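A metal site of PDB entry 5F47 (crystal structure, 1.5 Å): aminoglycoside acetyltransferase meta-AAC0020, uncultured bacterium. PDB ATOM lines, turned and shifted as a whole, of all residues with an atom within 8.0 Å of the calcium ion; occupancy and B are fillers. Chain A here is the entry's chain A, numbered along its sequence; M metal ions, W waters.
NE2 of Gln 49 lies within hydrogen-bond range of O of Glu 18, at 2.9 Å.
The side-chain amide oxygen (OD1) of Asn 53 lies within hydrogen-bond range of the side-chain amide nitrogen (NE2) of Gln 49 (2.9 Å).
The calcium ion is bound by the side-chain carboxylate (OE2) of Glu 18 (2.2 Å).
The calcium ion is bound by water W2 (2.3 Å).
The backbone carbonyl oxygen (O) of Asn 53 binds the calcium ion, 2.4 Å away.
Water W1 is bound to the calcium ion.
The calcium ion is bound by water W4 (2.5 Å).
OD1 of Asn 55 is bound to the calcium ion, 2.7 Å away.
Slightly farther from the calcium ion lies water W3 (3.0 Å).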
ATOM      1  N   ALA A  17       4.264   4.256 -19.003  1.00  0.00           N
ATOM      2  CA  ALA A  17       4.873   4.800 -20.198  1.00  0.00           C
ATOM      3  C   ALA A  17       4.651   6.307 -20.220  1.00  0.00           C
ATOM      4  O   ALA A  17       4.087   6.872 -19.282  1.00  0.00           O
ATOM      5  CB  ALA A  17       4.276   4.139 -21.432  1.00  0.00           C
ATOM      6  N   GLU A  18       5.075   6.958 -21.296  1.00  0.00           N
ATOM      7  CA  GLU A  18       5.047   8.422 -21.307  1.00  0.00           C
ATOM      8  C   GLU A  18       3.646   9.016 -21.338  1.00  0.00           C
ATOM      9  O   GLU A  18       3.463  10.165 -20.975  1.00  0.00           O
ATOM     10  CB  GLU A  18       5.864   8.944 -22.496  1.00  0.00           C
ATOM     11  CG  GLU A  18       7.369   8.713 -22.326  1.00  0.00           C
ATOM     12  CD  GLU A  18       8.196   9.394 -23.394  1.00  0.00           C
ATOM     13  OE1 GLU A  18       7.660  10.184 -24.200  1.00  0.00           O
ATOM     14  OE2 GLU A  18       9.401   9.119 -23.446  1.00  0.00           O
ATOM     15  N   GLN A  49       5.868  15.343 -16.079  1.00  0.00           N
ATOM     16  CA  GLN A  49       5.899  14.750 -17.419  1.00  0.00           C
ATOM     17  C   GLN A  49       7.315  14.638 -17.973  1.00  0.00           C
ATOM     18  O   GLN A  49       7.677  13.628 -18.585  1.00  0.00           O
ATOM     19  CB  GLN A  49       5.029  15.553 -18.389  1.00  0.00           C
ATOM     20  CG  GLN A  49       4.903  14.914 -19.799  1.00  0.00           C
ATOM     21  CD  GLN A  49       4.111  13.619 -19.778  1.00  0.00           C
ATOM     22  OE1 GLN A  49       2.900  13.632 -19.554  1.00  0.00           O
ATOM     23  NE2 GLN A  49       4.783  12.517 -20.029  1.00  0.00           N
ATOM     24  N   LYS A  50       8.136  15.650 -17.768  1.00  0.00           N
ATOM     25  CA  LYS A  50       9.525  15.600 -18.219  1.00  0.00           C
ATOM     26  C   LYS A  50      10.260  14.449 -17.557  1.00  0.00           C
ATOM     27  O   LYS A  50      11.059  13.749 -18.193  1.00  0.00           O
ATOM     28  CB  LYS A  50      10.261  16.909 -17.926  1.00  0.00           C
ATOM     29  CG  LYS A  50       9.853  18.045 -18.832  1.00  0.00           C
ATOM     30  CD  LYS A  50      10.573  19.306 -18.426  1.00  0.00           C
ATOM     31  CE  LYS A  50      10.215  20.436 -19.362  1.00  0.00           C
ATOM     32  NZ  LYS A  50      10.657  20.146 -20.744  1.00  0.00           N
ATOM     33  N   LEU A  51      10.000  14.252 -16.270  1.00  0.00           N
ATOM     34  CA  LEU A  51      10.620  13.151 -15.558  1.00  0.00           C
ATOM     35  C   LEU A  51      10.157  11.812 -16.130  1.00  0.00           C
ATOM     36  O   LEU A  51      10.977  10.923 -16.364  1.00  0.00           O
ATOM     37  CB  LEU A  51      10.301  13.255 -14.060  1.00  0.00           C
ATOM     38  CG  LEU A  51      10.755  12.113 -13.155  1.00  0.00           C
ATOM     39  CD1 LEU A  51      12.221  11.810 -13.388  1.00  0.00           C
ATOM     40  CD2 LEU A  51      10.516  12.536 -11.712  1.00  0.00           C
ATOM     41  N   LEU A  52       8.862  11.694 -16.393  1.00  0.00           N
ATOM     42  CA  LEU A  52       8.316  10.441 -16.876  1.00  0.00           C
ATOM     43  C   LEU A  52       8.896  10.133 -18.262  1.00  0.00           C
ATOM     44  O   LEU A  52       9.041   8.957 -18.651  1.00  0.00           O
ATOM     45  CB  LEU A  52       6.789  10.518 -16.892  1.00  0.00           C
ATOM     46  CG  LEU A  52       5.983   9.233 -17.087  1.00  0.00           C
ATOM     47  CD1 LEU A  52       6.265   8.250 -15.956  1.00  0.00           C
ATOM     48  CD2 LEU A  52       4.511   9.564 -17.161  1.00  0.00           C
ATOM     49  N   ASN A  53       9.277  11.190 -18.982  1.00  0.00           N
ATOM     50  CA  ASN A  53       9.816  11.047 -20.346  1.00  0.00           C
ATOM     51  C   ASN A  53      11.313  10.710 -20.376  1.00  0.00           C
ATOM     52  O   ASN A  53      11.861  10.407 -21.459  1.00  0.00           O
ATOM     53  CB  ASN A  53       9.559  12.335 -21.141  1.00  0.00           C
ATOM     54  CG  ASN A  53       8.078  12.528 -21.515  1.00  0.00           C
ATOM     55  OD1 ASN A  53       7.230  11.669 -21.261  1.00  0.00           O
ATOM     56  ND2 ASN A  53       7.757  13.693 -22.039  1.00  0.00           N
ATOM     57  N   GLN A  54      11.970  10.727 -19.209  1.00  0.00           N
ATOM     58  CA  GLN A  54      13.412  10.446 -19.153  1.00  0.00           C
ATOM     59  C   GLN A  54      13.674   8.982 -19.476  1.00  0.00           C
ATOM     60  O   GLN A  54      12.939   8.106 -19.016  1.00  0.00           O
ATOM     61  CB  GLN A  54      13.987  10.785 -17.771  1.00  0.00           C
ATOM     62  CG  GLN A  54      13.916  12.260 -17.488  1.00  0.00           C
ATOM     63  CD  GLN A  54      14.589  12.688 -16.201  1.00  0.00           C
ATOM     64  OE1 GLN A  54      14.426  13.832 -15.771  1.00  0.00           O
ATOM     65  NE2 GLN A  54      15.351  11.789 -15.565  1.00  0.00           N
ATOM     66  N   ASN A  55      14.754   8.703 -20.193  1.00  0.00           N
ATOM     67  CA  ASN A  55      15.070   7.310 -20.495  1.00  0.00           C
ATOM     68  C   ASN A  55      15.801   6.588 -19.372  1.00  0.00           C
ATOM     69  O   ASN A  55      16.142   5.415 -19.515  1.00  0.00           O
ATOM     70  CB  ASN A  55      15.865   7.216 -21.791  1.00  0.00           C
ATOM     71  CG  ASN A  55      15.022   7.552 -23.011  1.00  0.00           C
ATOM     72  OD1 ASN A  55      13.789   7.451 -22.974  1.00  0.00           O
ATOM     73  ND2 ASN A  55      15.678   7.922 -24.099  1.00  0.00           N
ATOM     74  N   ASN A  56      16.034   7.259 -18.241  1.00  0.00           N
ATOM     75  CA  ASN A  56      16.686   6.642 -17.093  1.00  0.00           C
ATOM     76  C   ASN A  56      15.751   6.486 -15.892  1.00  0.00           C
ATOM     77  O   ASN A  56      16.215   6.377 -14.771  1.00  0.00           O
ATOM     78  CB  ASN A  56      17.904   7.463 -16.651  1.00  0.00           C
ATOM     79  CG  ASN A  56      17.496   8.777 -16.018  1.00  0.00           C
ATOM     80  OD1 ASN A  56      16.392   9.247 -16.232  1.00  0.00           O
ATOM     81  ND2 ASN A  56      18.404   9.383 -15.230  1.00  0.00           N
ATOM     82  N   PHE A  57      14.438   6.512 -16.137  1.00  0.00           N
ATOM     83  CA  PHE A  57      13.466   6.500 -15.049  1.00  0.00           C
ATOM     84  C   PHE A  57      12.315   5.574 -15.418  1.00  0.00           C
ATOM     85  O   PHE A  57      11.740   5.700 -16.489  1.00  0.00           O
ATOM     86  CB  PHE A  57      12.971   7.929 -14.791  1.00  0.00           C
ATOM     87  CG  PHE A  57      12.019   8.080 -13.615  1.00  0.00           C
ATOM     88  CD1 PHE A  57      12.472   7.910 -12.288  1.00  0.00           C
ATOM     89  CD2 PHE A  57      10.706   8.404 -13.840  1.00  0.00           C
ATOM     90  CE1 PHE A  57      11.599   8.078 -11.224  1.00  0.00           C
ATOM     91  CE2 PHE A  57       9.817   8.585 -12.785  1.00  0.00           C
ATOM     92  CZ  PHE A  57      10.270   8.403 -11.465  1.00  0.00           C
ATOM     93  N   TYR A  58      12.016   4.631 -14.524  1.00  0.00           N
ATOM     94  CA  TYR A  58      10.918   3.691 -14.765  1.00  0.00           C
ATOM     95  C   TYR A  58      10.071   3.534 -13.517  1.00  0.00           C
ATOM     96  O   TYR A  58      10.584   3.325 -12.403  1.00  0.00           O
ATOM     97  CB  TYR A  58      11.449   2.317 -15.189  1.00  0.00           C
ATOM     98  CG  TYR A  58      12.003   2.263 -16.594  1.00  0.00           C
ATOM     99  CD1 TYR A  58      11.156   2.239 -17.685  1.00  0.00           C
ATOM    100  CD2 TYR A  58      13.386   2.218 -16.811  1.00  0.00           C
ATOM    101  CE1 TYR A  58      11.660   2.175 -18.975  1.00  0.00           C
ATOM    102  CE2 TYR A  58      13.895   2.158 -18.093  1.00  0.00           C
ATOM    103  CZ  TYR A  58      13.034   2.138 -19.164  1.00  0.00           C
ATOM    104  OH  TYR A  58      13.527   2.067 -20.456  1.00  0.00           O
HETATM  105 CA    CA M   1      11.537   8.920 -23.274  1.00  0.00          CA
HETATM  106  O   HOH W   1      11.211   8.287 -25.629  1.00  0.00           O
HETATM  107  O   HOH W   2      11.055   6.711 -23.196  1.00  0.00           O
HETATM  108  O   HOH W   3      10.436   7.613 -20.827  1.00  0.00           O
HETATM  109  O   HOH W   4      12.289  11.181 -24.032  1.00  0.00           O
